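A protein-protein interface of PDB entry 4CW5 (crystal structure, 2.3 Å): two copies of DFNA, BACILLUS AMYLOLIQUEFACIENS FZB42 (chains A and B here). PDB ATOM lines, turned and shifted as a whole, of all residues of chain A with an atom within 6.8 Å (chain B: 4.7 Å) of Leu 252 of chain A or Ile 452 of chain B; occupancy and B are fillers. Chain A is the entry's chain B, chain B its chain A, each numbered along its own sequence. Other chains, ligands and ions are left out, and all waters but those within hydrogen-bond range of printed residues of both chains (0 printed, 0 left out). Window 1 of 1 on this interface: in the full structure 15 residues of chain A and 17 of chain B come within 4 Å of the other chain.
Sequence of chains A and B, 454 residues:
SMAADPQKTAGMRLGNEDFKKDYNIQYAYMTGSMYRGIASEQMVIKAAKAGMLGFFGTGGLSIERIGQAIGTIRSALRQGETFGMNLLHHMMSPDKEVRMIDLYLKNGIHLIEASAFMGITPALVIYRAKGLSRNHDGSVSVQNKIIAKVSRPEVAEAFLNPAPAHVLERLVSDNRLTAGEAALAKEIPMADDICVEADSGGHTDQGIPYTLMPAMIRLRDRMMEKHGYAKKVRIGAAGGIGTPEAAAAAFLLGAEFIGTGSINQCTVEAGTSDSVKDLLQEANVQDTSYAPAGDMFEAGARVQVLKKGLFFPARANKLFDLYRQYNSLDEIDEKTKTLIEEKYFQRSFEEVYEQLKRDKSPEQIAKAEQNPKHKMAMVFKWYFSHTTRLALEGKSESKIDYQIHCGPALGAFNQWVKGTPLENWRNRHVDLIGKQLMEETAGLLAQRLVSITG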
ATOM      1  N   ALA A  10      -4.299 -33.054  -4.067  1.00  0.00           N
ATOM      2  CA  ALA A  10      -5.643 -32.675  -4.477  1.00  0.00           C
ATOM      3  C   ALA A  10      -6.378 -31.995  -3.326  1.00  0.00           C
ATOM      4  O   ALA A  10      -7.120 -31.037  -3.533  1.00  0.00           O
ATOM      5  CB  ALA A  10      -6.414 -33.896  -4.953  1.00  0.00           C
ATOM      6  N   ARG A  13      -5.534 -28.387  -3.163  1.00  0.00           N
ATOM      7  CA  ARG A  13      -6.008 -27.554  -4.265  1.00  0.00           C
ATOM      8  C   ARG A  13      -7.416 -27.031  -4.003  1.00  0.00           C
ATOM      9  O   ARG A  13      -7.825 -26.023  -4.582  1.00  0.00           O
ATOM     10  CB  ARG A  13      -5.988 -28.319  -5.589  1.00  0.00           C
ATOM     11  CG  ARG A  13      -4.608 -28.431  -6.227  1.00  0.00           C
ATOM     12  CD  ARG A  13      -4.690 -28.679  -7.733  1.00  0.00           C
ATOM     13  NE  ARG A  13      -5.943 -29.316  -8.135  1.00  0.00           N
ATOM     14  CZ  ARG A  13      -6.152 -30.629  -8.167  1.00  0.00           C
ATOM     15  NH1 ARG A  13      -5.188 -31.477  -7.827  1.00  0.00           N
ATOM     16  NH2 ARG A  13      -7.333 -31.097  -8.546  1.00  0.00           N
ATOM     17  N   LEU A  14      -8.155 -27.717  -3.134  1.00  0.00           N
ATOM     18  CA  LEU A  14      -9.529 -27.330  -2.825  1.00  0.00           C
ATOM     19  C   LEU A  14      -9.601 -25.938  -2.208  1.00  0.00           C
ATOM     20  O   LEU A  14      -8.682 -25.499  -1.516  1.00  0.00           O
ATOM     21  CB  LEU A  14     -10.181 -28.340  -1.872  1.00  0.00           C
ATOM     22  CG  LEU A  14     -10.441 -29.765  -2.378  1.00  0.00           C
ATOM     23  CD1 LEU A  14     -11.070 -30.604  -1.278  1.00  0.00           C
ATOM     24  CD2 LEU A  14     -11.330 -29.766  -3.613  1.00  0.00           C
ATOM     25  N   GLY A  15     -10.704 -25.250  -2.474  1.00  0.00           N
ATOM     26  CA  GLY A  15     -11.004 -23.985  -1.832  1.00  0.00           C
ATOM     27  C   GLY A  15     -10.195 -22.824  -2.368  1.00  0.00           C
ATOM     28  O   GLY A  15      -9.385 -22.980  -3.277  1.00  0.00           O
ATOM     29  N   ALA A 247     -18.377 -32.774   3.238  1.00  0.00           N
ATOM     30  CA  ALA A 247     -17.423 -31.731   2.892  1.00  0.00           C
ATOM     31  C   ALA A 247     -17.536 -31.400   1.412  1.00  0.00           C
ATOM     32  O   ALA A 247     -17.451 -30.237   1.014  1.00  0.00           O
ATOM     33  CB  ALA A 247     -16.011 -32.167   3.233  1.00  0.00           C
ATOM     34  N   ALA A 248     -17.748 -32.435   0.607  1.00  0.00           N
ATOM     35  CA  ALA A 248     -17.907 -32.278  -0.830  1.00  0.00           C
ATOM     36  C   ALA A 248     -19.153 -31.457  -1.125  1.00  0.00           C
ATOM     37  O   ALA A 248     -19.154 -30.609  -2.015  1.00  0.00           O
ATOM     38  CB  ALA A 248     -17.987 -33.639  -1.507  1.00  0.00           C
ATOM     39  N   ALA A 249     -20.208 -31.713  -0.360  1.00  0.00           N
ATOM     40  CA  ALA A 249     -21.465 -31.001  -0.526  1.00  0.00           C
ATOM     41  C   ALA A 249     -21.270 -29.522  -0.226  1.00  0.00           C
ATOM     42  O   ALA A 249     -21.789 -28.665  -0.937  1.00  0.00           O
ATOM     43  CB  ALA A 249     -22.536 -31.593   0.379  1.00  0.00           C
ATOM     44  N   ALA A 250     -20.516 -29.231   0.826  1.00  0.00           N
ATOM     45  CA  ALA A 250     -20.264 -27.853   1.222  1.00  0.00           C
ATOM     46  C   ALA A 250     -19.534 -27.092   0.120  1.00  0.00           C
ATOM     47  O   ALA A 250     -19.887 -25.955  -0.188  1.00  0.00           O
ATOM     48  CB  ALA A 250     -19.466 -27.812   2.517  1.00  0.00           C
ATOM     49  N   PHE A 251     -18.532 -27.725  -0.486  1.00  0.00           N
ATOM     50  CA  PHE A 251     -17.781 -27.089  -1.566  1.00  0.00           C
ATOM     51  C   PHE A 251     -18.653 -26.917  -2.808  1.00  0.00           C
ATOM     52  O   PHE A 251     -18.554 -25.905  -3.499  1.00  0.00           O
ATOM     53  CB  PHE A 251     -16.522 -27.891  -1.915  1.00  0.00           C
ATOM     54  CG  PHE A 251     -15.376 -27.674  -0.962  1.00  0.00           C
ATOM     55  CD1 PHE A 251     -14.699 -26.466  -0.936  1.00  0.00           C
ATOM     56  CD2 PHE A 251     -14.960 -28.686  -0.112  1.00  0.00           C
ATOM     57  CE1 PHE A 251     -13.643 -26.263  -0.064  1.00  0.00           C
ATOM     58  CE2 PHE A 251     -13.902 -28.490   0.758  1.00  0.00           C
ATOM     59  CZ  PHE A 251     -13.244 -27.276   0.782  1.00  0.00           C
ATOM     60  N   LEU A 252     -19.502 -27.901  -3.092  1.00  0.00           N
ATOM     61  CA  LEU A 252     -20.434 -27.797  -4.213  1.00  0.00           C
ATOM     62  C   LEU A 252     -21.343 -26.591  -4.041  1.00  0.00           C
ATOM     63  O   LEU A 252     -21.614 -25.859  -4.990  1.00  0.00           O
ATOM     64  CB  LEU A 252     -21.291 -29.058  -4.338  1.00  0.00           C
ATOM     65  CG  LEU A 252     -22.278 -29.049  -5.515  1.00  0.00           C
ATOM     66  CD1 LEU A 252     -21.567 -29.297  -6.832  1.00  0.00           C
ATOM     67  CD2 LEU A 252     -23.405 -30.053  -5.300  1.00  0.00           C
ATOM     68  N   LEU A 253     -21.817 -26.399  -2.816  1.00  0.00           N
ATOM     69  CA  LEU A 253     -22.726 -25.306  -2.508  1.00  0.00           C
ATOM     70  C   LEU A 253     -22.027 -23.944  -2.467  1.00  0.00           C
ATOM     71  O   LEU A 253     -22.684 -22.919  -2.286  1.00  0.00           O
ATOM     72  CB  LEU A 253     -23.433 -25.585  -1.181  1.00  0.00           C
ATOM     73  CG  LEU A 253     -24.400 -26.775  -1.208  1.00  0.00           C
ATOM     74  CD1 LEU A 253     -24.953 -27.041   0.182  1.00  0.00           C
ATOM     75  CD2 LEU A 253     -25.537 -26.576  -2.207  1.00  0.00           C
ATOM     76  N   GLY A 254     -20.704 -23.934  -2.638  1.00  0.00           N
ATOM     77  CA  GLY A 254     -19.961 -22.690  -2.769  1.00  0.00           C
ATOM     78  C   GLY A 254     -19.000 -22.325  -1.650  1.00  0.00           C
ATOM     79  O   GLY A 254     -18.413 -21.241  -1.674  1.00  0.00           O
ATOM     80  N   ALA A 255     -18.853 -23.198  -0.658  1.00  0.00           N
ATOM     81  CA  ALA A 255     -17.868 -22.983   0.401  1.00  0.00           C
ATOM     82  C   ALA A 255     -16.470 -22.819  -0.189  1.00  0.00           C
ATOM     83  O   ALA A 255     -16.025 -23.637  -0.990  1.00  0.00           O
ATOM     84  CB  ALA A 255     -17.891 -24.128   1.396  1.00  0.00           C
ATOM     85  N   LEU A 445     -14.902 -35.823  -4.964  1.00  0.00           N
ATOM     86  CA  LEU A 445     -15.357 -34.766  -5.857  1.00  0.00           C
ATOM     87  C   LEU A 445     -14.963 -35.074  -7.304  1.00  0.00           C
ATOM     88  O   LEU A 445     -15.774 -34.959  -8.221  1.00  0.00           O
ATOM     89  CB  LEU A 445     -14.757 -33.429  -5.422  1.00  0.00           C
ATOM     90  CG  LEU A 445     -15.548 -32.586  -4.415  1.00  0.00           C
ATOM     91  CD1 LEU A 445     -14.750 -31.342  -4.084  1.00  0.00           C
ATOM     92  CD2 LEU A 445     -16.942 -32.211  -4.889  1.00  0.00           C
ATOM     93  N   ALA B 248     -28.386 -31.429  -7.114  1.00  0.00           N
ATOM     94  CA  ALA B 248     -26.968 -31.654  -7.346  1.00  0.00           C
ATOM     95  C   ALA B 248     -26.302 -32.161  -6.072  1.00  0.00           C
ATOM     96  O   ALA B 248     -25.469 -33.065  -6.110  1.00  0.00           O
ATOM     97  CB  ALA B 248     -26.297 -30.376  -7.824  1.00  0.00           C
ATOM     98  N   ALA B 249     -26.688 -31.583  -4.941  1.00  0.00           N
ATOM     99  CA  ALA B 249     -26.121 -31.980  -3.660  1.00  0.00           C
ATOM    100  C   ALA B 249     -26.473 -33.432  -3.358  1.00  0.00           C
ATOM    101  O   ALA B 249     -25.622 -34.200  -2.914  1.00  0.00           O
ATOM    102  CB  ALA B 249     -26.620 -31.069  -2.547  1.00  0.00           C
ATOM    103  N   LEU B 252     -24.393 -35.751  -5.519  1.00  0.00           N
ATOM    104  CA  LEU B 252     -23.014 -35.699  -5.052  1.00  0.00           C
ATOM    105  C   LEU B 252     -22.872 -36.554  -3.798  1.00  0.00           C
ATOM    106  O   LEU B 252     -21.882 -37.257  -3.625  1.00  0.00           O
ATOM    107  CB  LEU B 252     -22.576 -34.260  -4.772  1.00  0.00           C
ATOM    108  CG  LEU B 252     -21.096 -34.120  -4.411  1.00  0.00           C
ATOM    109  CD1 LEU B 252     -20.256 -34.272  -5.667  1.00  0.00           C
ATOM    110  CD2 LEU B 252     -20.809 -32.796  -3.728  1.00  0.00           C
ATOM    111  N   LEU B 444     -25.220 -27.896 -13.702  1.00  0.00           N
ATOM    112  CA  LEU B 444     -24.679 -27.334 -12.473  1.00  0.00           C
ATOM    113  C   LEU B 444     -23.569 -28.210 -11.891  1.00  0.00           C
ATOM    114  O   LEU B 444     -22.492 -27.708 -11.563  1.00  0.00           O
ATOM    115  CB  LEU B 444     -25.803 -27.138 -11.455  1.00  0.00           C
ATOM    116  CG  LEU B 444     -25.479 -26.291 -10.220  1.00  0.00           C
ATOM    117  CD1 LEU B 444     -26.743 -25.651  -9.678  1.00  0.00           C
ATOM    118  CD2 LEU B 444     -24.808 -27.117  -9.132  1.00  0.00           C
ATOM    119  N   LEU B 445     -23.827 -29.511 -11.765  1.00  0.00           N
ATOM    120  CA  LEU B 445     -22.824 -30.425 -11.221  1.00  0.00           C
ATOM    121  C   LEU B 445     -21.534 -30.416 -12.015  1.00  0.00           C
ATOM    122  O   LEU B 445     -20.451 -30.326 -11.445  1.00  0.00           O
ATOM    123  CB  LEU B 445     -23.338 -31.864 -11.178  1.00  0.00           C
ATOM    124  CG  LEU B 445     -23.842 -32.459  -9.869  1.00  0.00           C
ATOM    125  CD1 LEU B 445     -24.347 -33.866 -10.117  1.00  0.00           C
ATOM    126  CD2 LEU B 445     -22.715 -32.489  -8.844  1.00  0.00           C
ATOM    127  N   ARG B 448     -19.651 -26.915 -11.781  1.00  0.00           N
ATOM    128  CA  ARG B 448     -19.077 -26.620 -10.473  1.00  0.00           C
ATOM    129  C   ARG B 448     -17.958 -27.582 -10.090  1.00  0.00           C
ATOM    130  O   ARG B 448     -16.948 -27.163  -9.526  1.00  0.00           O
ATOM    131  CB  ARG B 448     -20.171 -26.626  -9.403  1.00  0.00           C
ATOM    132  CG  ARG B 448     -21.004 -25.353  -9.412  1.00  0.00           C
ATOM    133  CD  ARG B 448     -21.894 -25.217  -8.193  1.00  0.00           C
ATOM    134  NE  ARG B 448     -22.830 -24.104  -8.341  1.00  0.00           N
ATOM    135  CZ  ARG B 448     -23.793 -23.806  -7.473  1.00  0.00           C
ATOM    136  NH1 ARG B 448     -23.964 -24.538  -6.381  1.00  0.00           N
ATOM    137  NH2 ARG B 448     -24.592 -22.772  -7.700  1.00  0.00           N
ATOM    138  N   LEU B 449     -18.130 -28.866 -10.392  1.00  0.00           N
ATOM    139  CA  LEU B 449     -17.086 -29.848 -10.113  1.00  0.00           C
ATOM    140  C   LEU B 449     -15.824 -29.529 -10.915  1.00  0.00           C
ATOM    141  O   LEU B 449     -14.710 -29.767 -10.452  1.00  0.00           O
ATOM    142  CB  LEU B 449     -17.569 -31.265 -10.420  1.00  0.00           C
ATOM    143  CG  LEU B 449     -18.615 -31.852  -9.466  1.00  0.00           C
ATOM    144  CD1 LEU B 449     -19.070 -33.213  -9.964  1.00  0.00           C
ATOM    145  CD2 LEU B 449     -18.086 -31.959  -8.043  1.00  0.00           C
ATOM    146  N   VAL B 450     -16.006 -28.987 -12.115  1.00  0.00           N
ATOM    147  CA  VAL B 450     -14.883 -28.569 -12.945  1.00  0.00           C
ATOM    148  C   VAL B 450     -14.176 -27.407 -12.258  1.00  0.00           C
ATOM    149  O   VAL B 450     -12.954 -27.394 -12.114  1.00  0.00           O
ATOM    150  CB  VAL B 450     -15.346 -28.154 -14.360  1.00  0.00           C
ATOM    151  CG1 VAL B 450     -14.376 -27.150 -15.000  1.00  0.00           C
ATOM    152  CG2 VAL B 450     -15.511 -29.377 -15.239  1.00  0.00           C
ATOM    153  N   SER B 451     -14.974 -26.418 -11.874  1.00  0.00           N
ATOM    154  CA  SER B 451     -14.498 -25.254 -11.143  1.00  0.00           C
ATOM    155  C   SER B 451     -13.764 -25.635  -9.854  1.00  0.00           C
ATOM    156  O   SER B 451     -12.709 -25.085  -9.549  1.00  0.00           O
ATOM    157  CB  SER B 451     -15.669 -24.326 -10.824  1.00  0.00           C
ATOM    158  OG  SER B 451     -15.204 -23.071 -10.368  1.00  0.00           O
ATOM    159  N   ILE B 452     -14.325 -26.582  -9.103  1.00  0.00           N
ATOM    160  CA  ILE B 452     -13.840 -26.880  -7.757  1.00  0.00           C
ATOM    161  C   ILE B 452     -12.603 -27.774  -7.741  1.00  0.00           C
ATOM    162  O   ILE B 452     -11.781 -27.673  -6.829  1.00  0.00           O
ATOM    163  CB  ILE B 452     -14.946 -27.594  -6.928  1.00  0.00           C
ATOM    164  CG1 ILE B 452     -16.093 -26.643  -6.599  1.00  0.00           C
ATOM    165  CG2 ILE B 452     -14.389 -28.189  -5.625  1.00  0.00           C
ATOM    166  CD1 ILE B 452     -17.374 -27.366  -6.208  1.00  0.00           C
ATOM    167  N   THR B 453     -12.457 -28.621  -8.755  1.00  0.00           N
ATOM    168  CA  THR B 453     -11.326 -29.546  -8.821  1.00  0.00           C
ATOM    169  C   THR B 453     -10.283 -29.104  -9.845  1.00  0.00           C
ATOM    170  O   THR B 453      -9.269 -29.773 -10.030  1.00  0.00           O
ATOM    171  CB  THR B 453     -11.794 -30.979  -9.164  1.00  0.00           C
ATOM    172  OG1 THR B 453     -12.448 -30.996 -10.439  1.00  0.00           O
ATOM    173  CG2 THR B 453     -12.747 -31.497  -8.097  1.00  0.00           C
ATOM    174  N   GLY B 454     -10.539 -27.982 -10.508  1.00  0.00           N
ATOM    175  CA  GLY B 454      -9.643 -27.471 -11.531  1.00  0.00           C
ATOM    176  C   GLY B 454      -8.283 -27.060 -11.001  1.00  0.00           C
ATOM    177  O   GLY B 454      -7.471 -26.505 -11.741  1.00  0.00           O
ATOM    178  OXT GLY B 454      -7.956 -27.260  -9.830  1.00  0.00           O
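NH1 of Arg 448 of chain B is in hydrogen-bond range of O of Leu 252 of chain A.
The guanidinium group of Arg 13 of chain A is in hydrogen-bond range of the backbone carbonyl oxygen of Thr 453 of chain B, 2.8 Å away.
The chain-end carboxylate of Gly 454 of chain B lies within salt-bridge range of the guanidinium group of Arg 13 of chain A, 3.3 Å away.
The backbone carbonyl oxygen (O) of Leu 449 of chain B sits at hydrogen-bond distance from the side-chain hydroxyl (OG1) of Thr 453 of chain B (2.6 Å).
Among the printed residues, pairs that only touch across the chains: Ala 248 of chain A with Leu 252 of chain B (3.2 Å), Phe 251 of chain A with Ile 452 of chain B (3.3 Å), Leu 445 of chain A with Leu 449 of chain B (3.4 Å), Leu 445 of chain A with Ile 452 of chain B (3.5 Å), Ala 249 of chain A with Leu 252 of chain B (3.6 Å), Leu 252 of chain A with Ala 249 of chain B (3.6 Å), Leu 252 of chain A with Ala 248 of chain B (3.7 Å), Leu 252 of chain A with Ile 452 of chain B (3.7 Å), Leu 252 of chain A with Leu 252 of chain B (3.8 Å), Leu 14 of chain A with Ile 452 of chain B (3.9 Å), Leu 445 of chain A with Thr 453 of chain B (3.9 Å), Leu 252 of chain A with Leu 445 of chain B (3.9 Å) and Leu 445 of chain A with Leu 252 of chain B (3.98 Å).
Of chain B, only Ala 248, Ala 249, Leu 252, Leu 445, Arg 448 and Ile 452 come within 4 Å of Leu 252 of chain A.
Ile 452 of chain B touches just these residues of chain A: Leu 14 (3.9 Å), Phe 251 (3.3 Å), Leu 252 (3.7 Å) and Leu 445 (3.5 Å).
Printed residues of chain B within 4 Å of Leu 14 of chain A: Ile 452.
Printed residues of chain A within 4 Å of Thr 453 of chain B: Arg 13 (2.8 Å) and Leu 445 (3.9 Å).
Of the printed residues of chain B, Ala 249 of chain A touches Leu 252.
Of the printed residues of chain A, Arg 448 of chain B touches Leu 252.
Leu 444 of chain B touches none of the printed residues of chain A.
The nearest printed residue of chain B that does not touch Leu 252 of chain A is Leu 444 of chain B (4.5 Å).
The nearest residue of chain A that does not touch Ile 452 of chain B is Arg 13 of chain A (4.8 Å).
The nearest printed residue of chain B that does not touch Arg 13 of chain A is Ile 452 of chain B (4.8 Å).
Printed residues of chain B that touch a printed residue of chain A: Ala 248, Ala 249, Leu 252, Leu 445, Arg 448, Leu 449, Ile 452, Thr 453 and Gly 454.
Hydrophobic or aromatic side chains of chain B within 4 Å of the printed part of chain A: Ala 248, Leu 252, Leu 445, Leu 449 and Ile 452.
Printed residues of chain A that touch a printed residue of chain B: Arg 13, Leu 14, Ala 248, Ala 249, Phe 251, Leu 252 and Leu 445.
Hydrophobic or aromatic side chains of chain A within 4 Å of the printed part of chain B: Leu 14, Ala 248, Leu 252 and Leu 445.
Among the printed residues, 16 pairs touch across the chains.
Among the printed residues, no Asp or Glu carboxylate lies within 4 Å of a Lys or Arg side-chain nitrogen of the other chain.
Ala 248 of chain A touches Leu 252 of chain B, and with the chains exchanged Leu 252 of chain A touches Ala 248 of chain B.
Ala 249 of chain A touches Leu 252 of chain B, and with the chains exchanged Leu 252 of chain A touches Ala 249 of chain B.
Leu 252 of chain A touches its own counterpart, Leu 252 of chain B.
Leu 252 of chain A touches Leu 445 of chain B, and with the chains exchanged Leu 445 of chain A touches Leu 252 of chain B.
Of the 16 pairs that touch across the chains among the printed residues, 7 have their exchanged pair printed and touching as well.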
